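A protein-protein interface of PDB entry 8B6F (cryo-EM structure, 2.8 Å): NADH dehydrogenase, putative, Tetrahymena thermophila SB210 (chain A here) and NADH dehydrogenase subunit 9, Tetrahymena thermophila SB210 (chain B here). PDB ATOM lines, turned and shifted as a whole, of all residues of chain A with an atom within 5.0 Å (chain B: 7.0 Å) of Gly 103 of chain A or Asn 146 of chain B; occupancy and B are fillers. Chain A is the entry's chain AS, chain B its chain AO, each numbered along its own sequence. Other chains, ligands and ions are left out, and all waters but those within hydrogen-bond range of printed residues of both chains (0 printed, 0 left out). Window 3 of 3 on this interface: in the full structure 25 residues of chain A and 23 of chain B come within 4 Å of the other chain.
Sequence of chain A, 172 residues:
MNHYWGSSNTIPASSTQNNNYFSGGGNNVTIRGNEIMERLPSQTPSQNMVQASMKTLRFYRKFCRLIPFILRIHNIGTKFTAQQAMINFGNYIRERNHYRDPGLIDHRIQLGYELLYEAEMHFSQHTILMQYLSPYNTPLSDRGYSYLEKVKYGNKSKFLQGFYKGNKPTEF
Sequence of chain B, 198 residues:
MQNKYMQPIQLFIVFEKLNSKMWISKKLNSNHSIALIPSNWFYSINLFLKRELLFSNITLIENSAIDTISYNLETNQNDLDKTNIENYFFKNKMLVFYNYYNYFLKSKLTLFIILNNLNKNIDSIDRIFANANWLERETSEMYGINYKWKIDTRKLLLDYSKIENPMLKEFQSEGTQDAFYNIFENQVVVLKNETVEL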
ATOM      1  N   SER A  46      10.544 -16.496 -17.821  1.00  0.00           N
ATOM      2  CA  SER A  46      10.074 -16.212 -16.471  1.00  0.00           C
ATOM      3  C   SER A  46       8.554 -16.272 -16.471  1.00  0.00           C
ATOM      4  O   SER A  46       7.900 -15.524 -17.205  1.00  0.00           O
ATOM      5  CB  SER A  46      10.568 -14.846 -15.997  1.00  0.00           C
ATOM      6  OG  SER A  46      10.194 -13.824 -16.904  1.00  0.00           O
ATOM      7  N   ASP A 101       4.815  -7.462 -17.733  1.00  0.00           N
ATOM      8  CA  ASP A 101       4.834  -8.544 -18.717  1.00  0.00           C
ATOM      9  C   ASP A 101       6.149  -9.304 -18.605  1.00  0.00           C
ATOM     10  O   ASP A 101       7.205  -8.761 -18.983  1.00  0.00           O
ATOM     11  CB  ASP A 101       4.657  -7.979 -20.125  1.00  0.00           C
ATOM     12  CG  ASP A 101       4.322  -9.046 -21.143  1.00  0.00           C
ATOM     13  OD1 ASP A 101       4.304 -10.239 -20.775  1.00  0.00           O
ATOM     14  OD2 ASP A 101       4.072  -8.692 -22.313  1.00  0.00           O
ATOM     15  N   PRO A 102       6.155 -10.541 -18.100  1.00  0.00           N
ATOM     16  CA  PRO A 102       7.437 -11.247 -17.933  1.00  0.00           C
ATOM     17  C   PRO A 102       8.235 -11.388 -19.217  1.00  0.00           C
ATOM     18  O   PRO A 102       9.465 -11.268 -19.188  1.00  0.00           O
ATOM     19  CB  PRO A 102       7.009 -12.612 -17.377  1.00  0.00           C
ATOM     20  CG  PRO A 102       5.709 -12.359 -16.716  1.00  0.00           C
ATOM     21  CD  PRO A 102       5.030 -11.305 -17.533  1.00  0.00           C
ATOM     22  N   GLY A 103       7.575 -11.641 -20.346  1.00  0.00           N
ATOM     23  CA  GLY A 103       8.304 -11.775 -21.596  1.00  0.00           C
ATOM     24  C   GLY A 103       8.976 -10.484 -22.016  1.00  0.00           C
ATOM     25  O   GLY A 103      10.137 -10.485 -22.432  1.00  0.00           O
ATOM     26  N   LEU A 104       8.258  -9.366 -21.918  1.00  0.00           N
ATOM     27  CA  LEU A 104       8.860  -8.075 -22.228  1.00  0.00           C
ATOM     28  C   LEU A 104      10.028  -7.778 -21.298  1.00  0.00           C
ATOM     29  O   LEU A 104      11.062  -7.258 -21.731  1.00  0.00           O
ATOM     30  CB  LEU A 104       7.806  -6.973 -22.134  1.00  0.00           C
ATOM     31  CG  LEU A 104       8.263  -5.568 -22.523  1.00  0.00           C
ATOM     32  CD1 LEU A 104       8.689  -5.515 -23.980  1.00  0.00           C
ATOM     33  CD2 LEU A 104       7.158  -4.566 -22.252  1.00  0.00           C
ATOM     34  N   ILE A 105       9.883  -8.107 -20.015  1.00  0.00           N
ATOM     35  CA  ILE A 105      10.963  -7.879 -19.060  1.00  0.00           C
ATOM     36  C   ILE A 105      12.181  -8.717 -19.422  1.00  0.00           C
ATOM     37  O   ILE A 105      13.320  -8.238 -19.361  1.00  0.00           O
ATOM     38  CB  ILE A 105      10.480  -8.164 -17.628  1.00  0.00           C
ATOM     39  CG1 ILE A 105       9.390  -7.165 -17.236  1.00  0.00           C
ATOM     40  CG2 ILE A 105      11.650  -8.081 -16.657  1.00  0.00           C
ATOM     41  CD1 ILE A 105       8.626  -7.543 -15.994  1.00  0.00           C
ATOM     42  N   ASP A 106      11.969  -9.975 -19.811  1.00  0.00           N
ATOM     43  CA  ASP A 106      13.095 -10.813 -20.214  1.00  0.00           C
ATOM     44  C   ASP A 106      13.799 -10.225 -21.426  1.00  0.00           C
ATOM     45  O   ASP A 106      15.033 -10.186 -21.478  1.00  0.00           O
ATOM     46  CB  ASP A 106      12.615 -12.231 -20.521  1.00  0.00           C
ATOM     47  CG  ASP A 106      11.908 -12.872 -19.348  1.00  0.00           C
ATOM     48  OD1 ASP A 106      11.830 -12.234 -18.279  1.00  0.00           O
ATOM     49  OD2 ASP A 106      11.426 -14.013 -19.495  1.00  0.00           O
ATOM     50  N   HIS A 107      13.033  -9.758 -22.411  1.00  0.00           N
ATOM     51  CA  HIS A 107      13.637  -9.137 -23.584  1.00  0.00           C
ATOM     52  C   HIS A 107      14.437  -7.902 -23.188  1.00  0.00           C
ATOM     53  O   HIS A 107      15.548  -7.686 -23.685  1.00  0.00           O
ATOM     54  CB  HIS A 107      12.545  -8.782 -24.593  1.00  0.00           C
ATOM     55  CG  HIS A 107      13.029  -8.692 -26.005  1.00  0.00           C
ATOM     56  ND1 HIS A 107      12.821  -7.580 -26.792  1.00  0.00           N
ATOM     57  CD2 HIS A 107      13.707  -9.575 -26.774  1.00  0.00           C
ATOM     58  CE1 HIS A 107      13.352  -7.781 -27.984  1.00  0.00           C
ATOM     59  NE2 HIS A 107      13.895  -8.984 -28.000  1.00  0.00           N
ATOM     60  N   GLN A 110      17.706  -8.948 -21.582  1.00  0.00           N
ATOM     61  CA  GLN A 110      18.656  -9.366 -22.606  1.00  0.00           C
ATOM     62  C   GLN A 110      19.312  -8.155 -23.254  1.00  0.00           C
ATOM     63  O   GLN A 110      20.535  -8.115 -23.427  1.00  0.00           O
ATOM     64  CB  GLN A 110      17.948 -10.220 -23.659  1.00  0.00           C
ATOM     65  CG  GLN A 110      17.435 -11.550 -23.140  1.00  0.00           C
ATOM     66  CD  GLN A 110      16.602 -12.283 -24.169  1.00  0.00           C
ATOM     67  OE1 GLN A 110      16.531 -11.879 -25.327  1.00  0.00           O
ATOM     68  NE2 GLN A 110      15.962 -13.366 -23.748  1.00  0.00           N
ATOM     69  N   LEU B 115       1.550 -14.653 -34.378  1.00  0.00           N
ATOM     70  CA  LEU B 115       1.847 -14.246 -33.010  1.00  0.00           C
ATOM     71  C   LEU B 115       0.797 -13.225 -32.596  1.00  0.00           C
ATOM     72  O   LEU B 115       0.755 -12.116 -33.139  1.00  0.00           O
ATOM     73  CB  LEU B 115       3.257 -13.670 -32.897  1.00  0.00           C
ATOM     74  CG  LEU B 115       4.386 -14.562 -33.414  1.00  0.00           C
ATOM     75  CD1 LEU B 115       5.715 -13.835 -33.347  1.00  0.00           C
ATOM     76  CD2 LEU B 115       4.447 -15.860 -32.629  1.00  0.00           C
ATOM     77  N   ASN B 119       3.774  -9.639 -26.354  1.00  0.00           N
ATOM     78  CA  ASN B 119       5.225  -9.675 -26.223  1.00  0.00           C
ATOM     79  C   ASN B 119       5.909 -10.423 -27.361  1.00  0.00           C
ATOM     80  O   ASN B 119       7.143 -10.407 -27.431  1.00  0.00           O
ATOM     81  CB  ASN B 119       5.618 -10.300 -24.880  1.00  0.00           C
ATOM     82  CG  ASN B 119       5.004 -11.667 -24.668  1.00  0.00           C
ATOM     83  OD1 ASN B 119       4.772 -12.412 -25.618  1.00  0.00           O
ATOM     84  ND2 ASN B 119       4.732 -12.001 -23.412  1.00  0.00           N
ATOM     85  N   LYS B 120       5.153 -11.070 -28.247  1.00  0.00           N
ATOM     86  CA  LYS B 120       5.709 -11.719 -29.432  1.00  0.00           C
ATOM     87  C   LYS B 120       6.687 -12.831 -29.048  1.00  0.00           C
ATOM     88  O   LYS B 120       7.854 -12.837 -29.441  1.00  0.00           O
ATOM     89  CB  LYS B 120       6.388 -10.689 -30.340  1.00  0.00           C
ATOM     90  CG  LYS B 120       5.530  -9.480 -30.677  1.00  0.00           C
ATOM     91  CD  LYS B 120       6.352  -8.424 -31.397  1.00  0.00           C
ATOM     92  CE  LYS B 120       5.585  -7.125 -31.551  1.00  0.00           C
ATOM     93  NZ  LYS B 120       6.423  -6.057 -32.159  1.00  0.00           N
ATOM     94  N   ASN B 121       6.186 -13.784 -28.268  1.00  0.00           N
ATOM     95  CA  ASN B 121       6.983 -14.918 -27.826  1.00  0.00           C
ATOM     96  C   ASN B 121       6.867 -16.071 -28.814  1.00  0.00           C
ATOM     97  O   ASN B 121       5.774 -16.396 -29.284  1.00  0.00           O
ATOM     98  CB  ASN B 121       6.540 -15.388 -26.439  1.00  0.00           C
ATOM     99  CG  ASN B 121       7.051 -14.493 -25.331  1.00  0.00           C
ATOM    100  OD1 ASN B 121       8.095 -13.859 -25.462  1.00  0.00           O
ATOM    101  ND2 ASN B 121       6.317 -14.444 -24.226  1.00  0.00           N
ATOM    102  N   ILE B 122       8.006 -16.680 -29.129  1.00  0.00           N
ATOM    103  CA  ILE B 122       8.044 -17.842 -30.007  1.00  0.00           C
ATOM    104  C   ILE B 122       9.349 -18.580 -29.751  1.00  0.00           C
ATOM    105  O   ILE B 122      10.382 -17.963 -29.482  1.00  0.00           O
ATOM    106  CB  ILE B 122       7.899 -17.430 -31.491  1.00  0.00           C
ATOM    107  CG1 ILE B 122       7.907 -18.674 -32.386  1.00  0.00           C
ATOM    108  CG2 ILE B 122       9.007 -16.462 -31.883  1.00  0.00           C
ATOM    109  CD1 ILE B 122       7.664 -18.390 -33.852  1.00  0.00           C
ATOM    110  N   ASP B 123       9.295 -19.907 -29.834  1.00  0.00           N
ATOM    111  CA  ASP B 123      10.487 -20.718 -29.633  1.00  0.00           C
ATOM    112  C   ASP B 123      11.419 -20.599 -30.832  1.00  0.00           C
ATOM    113  O   ASP B 123      10.986 -20.706 -31.983  1.00  0.00           O
ATOM    114  CB  ASP B 123      10.107 -22.182 -29.417  1.00  0.00           C
ATOM    115  CG  ASP B 123       9.438 -22.419 -28.081  1.00  0.00           C
ATOM    116  OD1 ASP B 123       9.783 -21.716 -27.109  1.00  0.00           O
ATOM    117  OD2 ASP B 123       8.566 -23.309 -28.003  1.00  0.00           O
ATOM    118  N   SER B 124      12.700 -20.378 -30.559  1.00  0.00           N
ATOM    119  CA  SER B 124      13.699 -20.319 -31.610  1.00  0.00           C
ATOM    120  C   SER B 124      14.055 -21.726 -32.088  1.00  0.00           C
ATOM    121  O   SER B 124      13.898 -22.714 -31.366  1.00  0.00           O
ATOM    122  CB  SER B 124      14.952 -19.600 -31.115  1.00  0.00           C
ATOM    123  OG  SER B 124      15.979 -19.633 -32.089  1.00  0.00           O
ATOM    124  N   SER B 140      14.346 -10.566 -34.650  1.00  0.00           N
ATOM    125  CA  SER B 140      14.039 -10.080 -33.311  1.00  0.00           C
ATOM    126  C   SER B 140      14.348  -8.597 -33.171  1.00  0.00           C
ATOM    127  O   SER B 140      13.548  -7.840 -32.611  1.00  0.00           O
ATOM    128  CB  SER B 140      14.829 -10.884 -32.279  1.00  0.00           C
ATOM    129  OG  SER B 140      14.659 -10.355 -30.977  1.00  0.00           O
ATOM    130  N   TYR B 143      11.905  -6.393 -35.679  1.00  0.00           N
ATOM    131  CA  TYR B 143      10.480  -6.453 -35.399  1.00  0.00           C
ATOM    132  C   TYR B 143      10.152  -6.670 -33.930  1.00  0.00           C
ATOM    133  O   TYR B 143       8.974  -6.601 -33.565  1.00  0.00           O
ATOM    134  CB  TYR B 143       9.822  -7.570 -36.225  1.00  0.00           C
ATOM    135  CG  TYR B 143       9.751  -7.269 -37.702  1.00  0.00           C
ATOM    136  CD1 TYR B 143       8.673  -6.574 -38.238  1.00  0.00           C
ATOM    137  CD2 TYR B 143      10.758  -7.679 -38.562  1.00  0.00           C
ATOM    138  CE1 TYR B 143       8.604  -6.297 -39.589  1.00  0.00           C
ATOM    139  CE2 TYR B 143      10.699  -7.409 -39.912  1.00  0.00           C
ATOM    140  CZ  TYR B 143       9.622  -6.717 -40.420  1.00  0.00           C
ATOM    141  OH  TYR B 143       9.562  -6.444 -41.765  1.00  0.00           O
ATOM    142  N   GLY B 144      11.143  -6.927 -33.082  1.00  0.00           N
ATOM    143  CA  GLY B 144      10.889  -7.075 -31.663  1.00  0.00           C
ATOM    144  C   GLY B 144      10.326  -8.412 -31.244  1.00  0.00           C
ATOM    145  O   GLY B 144       9.669  -8.491 -30.204  1.00  0.00           O
ATOM    146  N   ILE B 145      10.560  -9.470 -32.020  1.00  0.00           N
ATOM    147  CA  ILE B 145      10.098 -10.798 -31.633  1.00  0.00           C
ATOM    148  C   ILE B 145      10.982 -11.329 -30.515  1.00  0.00           C
ATOM    149  O   ILE B 145      12.215 -11.294 -30.606  1.00  0.00           O
ATOM    150  CB  ILE B 145      10.091 -11.746 -32.843  1.00  0.00           C
ATOM    151  CG1 ILE B 145       8.886 -11.475 -33.747  1.00  0.00           C
ATOM    152  CG2 ILE B 145      10.065 -13.207 -32.401  1.00  0.00           C
ATOM    153  CD1 ILE B 145       8.933 -10.160 -34.475  1.00  0.00           C
ATOM    154  N   ASN B 146      10.354 -11.824 -29.450  1.00  0.00           N
ATOM    155  CA  ASN B 146      11.072 -12.362 -28.298  1.00  0.00           C
ATOM    156  C   ASN B 146      11.290 -13.852 -28.528  1.00  0.00           C
ATOM    157  O   ASN B 146      10.509 -14.692 -28.085  1.00  0.00           O
ATOM    158  CB  ASN B 146      10.302 -12.100 -27.012  1.00  0.00           C
ATOM    159  CG  ASN B 146      10.934 -12.766 -25.808  1.00  0.00           C
ATOM    160  OD1 ASN B 146      12.129 -13.057 -25.800  1.00  0.00           O
ATOM    161  ND2 ASN B 146      10.133 -13.014 -24.780  1.00  0.00           N
ATOM    162  N   TYR B 147      12.364 -14.183 -29.239  1.00  0.00           N
ATOM    163  CA  TYR B 147      12.726 -15.579 -29.432  1.00  0.00           C
ATOM    164  C   TYR B 147      13.193 -16.192 -28.119  1.00  0.00           C
ATOM    165  O   TYR B 147      13.948 -15.578 -27.360  1.00  0.00           O
ATOM    166  CB  TYR B 147      13.818 -15.708 -30.490  1.00  0.00           C
ATOM    167  CG  TYR B 147      13.305 -15.601 -31.906  1.00  0.00           C
ATOM    168  CD1 TYR B 147      12.627 -16.657 -32.499  1.00  0.00           C
ATOM    169  CD2 TYR B 147      13.505 -14.452 -32.651  1.00  0.00           C
ATOM    170  CE1 TYR B 147      12.159 -16.566 -33.793  1.00  0.00           C
ATOM    171  CE2 TYR B 147      13.041 -14.350 -33.946  1.00  0.00           C
ATOM    172  CZ  TYR B 147      12.369 -15.411 -34.512  1.00  0.00           C
ATOM    173  OH  TYR B 147      11.906 -15.316 -35.802  1.00  0.00           O
ATOM    174  N   LYS B 148      12.746 -17.415 -27.858  1.00  0.00           N
ATOM    175  CA  LYS B 148      13.044 -18.126 -26.624  1.00  0.00           C
ATOM    176  C   LYS B 148      13.963 -19.300 -26.920  1.00  0.00           C
ATOM    177  O   LYS B 148      13.848 -19.942 -27.968  1.00  0.00           O
ATOM    178  CB  LYS B 148      11.760 -18.617 -25.955  1.00  0.00           C
ATOM    179  CG  LYS B 148      10.820 -17.498 -25.540  1.00  0.00           C
ATOM    180  CD  LYS B 148       9.372 -17.958 -25.551  1.00  0.00           C
ATOM    181  CE  LYS B 148       9.146 -19.132 -24.615  1.00  0.00           C
ATOM    182  NZ  LYS B 148       7.729 -19.583 -24.641  1.00  0.00           N
ATOM    183  N   TRP B 149      14.879 -19.573 -25.996  1.00  0.00           N
ATOM    184  CA  TRP B 149      15.823 -20.678 -26.137  1.00  0.00           C
ATOM    185  C   TRP B 149      16.730 -20.467 -27.347  1.00  0.00           C
ATOM    186  O   TRP B 149      17.112 -21.415 -28.035  1.00  0.00           O
ATOM    187  CB  TRP B 149      15.083 -22.012 -26.224  1.00  0.00           C
ATOM    188  CG  TRP B 149      14.115 -22.188 -25.102  1.00  0.00           C
ATOM    189  CD1 TRP B 149      12.759 -22.085 -25.164  1.00  0.00           C
ATOM    190  CD2 TRP B 149      14.436 -22.476 -23.737  1.00  0.00           C
ATOM    191  NE1 TRP B 149      12.212 -22.300 -23.922  1.00  0.00           N
ATOM    192  CE2 TRP B 149      13.223 -22.543 -23.029  1.00  0.00           C
ATOM    193  CE3 TRP B 149      15.634 -22.691 -23.048  1.00  0.00           C
ATOM    194  CZ2 TRP B 149      13.171 -22.816 -21.666  1.00  0.00           C
ATOM    195  CZ3 TRP B 149      15.581 -22.960 -21.695  1.00  0.00           C
ATOM    196  CH2 TRP B 149      14.358 -23.021 -21.017  1.00  0.00           C
ATOM    197  N   THR B 153      21.180 -13.941 -28.524  1.00  0.00           N
ATOM    198  CA  THR B 153      20.169 -12.901 -28.654  1.00  0.00           C
ATOM    199  C   THR B 153      20.755 -11.528 -28.956  1.00  0.00           C
ATOM    200  O   THR B 153      19.994 -10.568 -29.105  1.00  0.00           O
ATOM    201  CB  THR B 153      19.332 -12.816 -27.375  1.00  0.00           C
ATOM    202  OG1 THR B 153      20.184 -12.525 -26.260  1.00  0.00           O
ATOM    203  CG2 THR B 153      18.608 -14.122 -27.126  1.00  0.00           C
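The side-chain hydroxyl of Ser 140 of chain B sits at hydrogen-bond distance from a ring nitrogen (NE2) of His 107 of chain A (3.4 Å).
ND2 of Asn 146 of chain B is in hydrogen-bond range of O of Gly 103 of chain A, 3.5 Å away.
The side-chain amide nitrogen of Asn 119 of chain B lies within hydrogen-bond range of the side-chain carboxylate of Asp 101 of chain A, at 3.2 Å.
The backbone NH of Ile 122 of chain B sits at hydrogen-bond distance from the backbone carbonyl oxygen of Asn 146 of chain B.
The backbone carbonyl oxygen of Lys 120 of chain B sits at hydrogen-bond distance from the backbone NH of Asn 146 of chain B.
The side-chain hydroxyl of Ser 140 of chain B lies within hydrogen-bond range of the backbone carbonyl oxygen of Ile 145 of chain B (2.6 Å).
The side-chain amide oxygen of Asn 119 of chain B is in hydrogen-bond range of the side-chain amide nitrogen of Asn 121 of chain B.
Ile 145 of chain B touches His 107 of chain A (O to NE2, 3.9 Å).
His 107 of chain A touches Asn 146 of chain B (CD2 to OD1, 3.9 Å).
Thr 153 of chain B touches Gln 110 of chain A (CG2 to OE1, 3.5 Å).
Printed residues of chain B within 4 Å of Gly 103 of chain A: Asn 146 (3.5 Å).
Printed residues of chain A within 4 Å of Ile 145 of chain B: His 107.
Printed residues of chain A within 4 Å of Ser 140 of chain B: His 107 (3.4 Å).
Tyr 147 of chain B touches none of the printed residues of chain A.
Lys 120 of chain B touches none of the printed residues of chain A.
The nearest printed residue of chain B that does not touch Gly 103 of chain A is Asn 119 of chain B (4.01 Å).
The nearest printed residue of chain B that does not touch His 107 of chain A is Gly 144 of chain B (4.4 Å).
Of the 9 printed residues of chain A, 4 touch a printed residue of chain B.
Hydrophobic or aromatic side chains of chain A within 4 Å of the printed part of chain B: His 107.
Along chain A the printed residues that touch a printed residue of chain B span positions 101 to 110.
Among the printed residues, no Asp or Glu carboxylate lies within 4 Å of a Lys or Arg side-chain nitrogen of the other chain.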
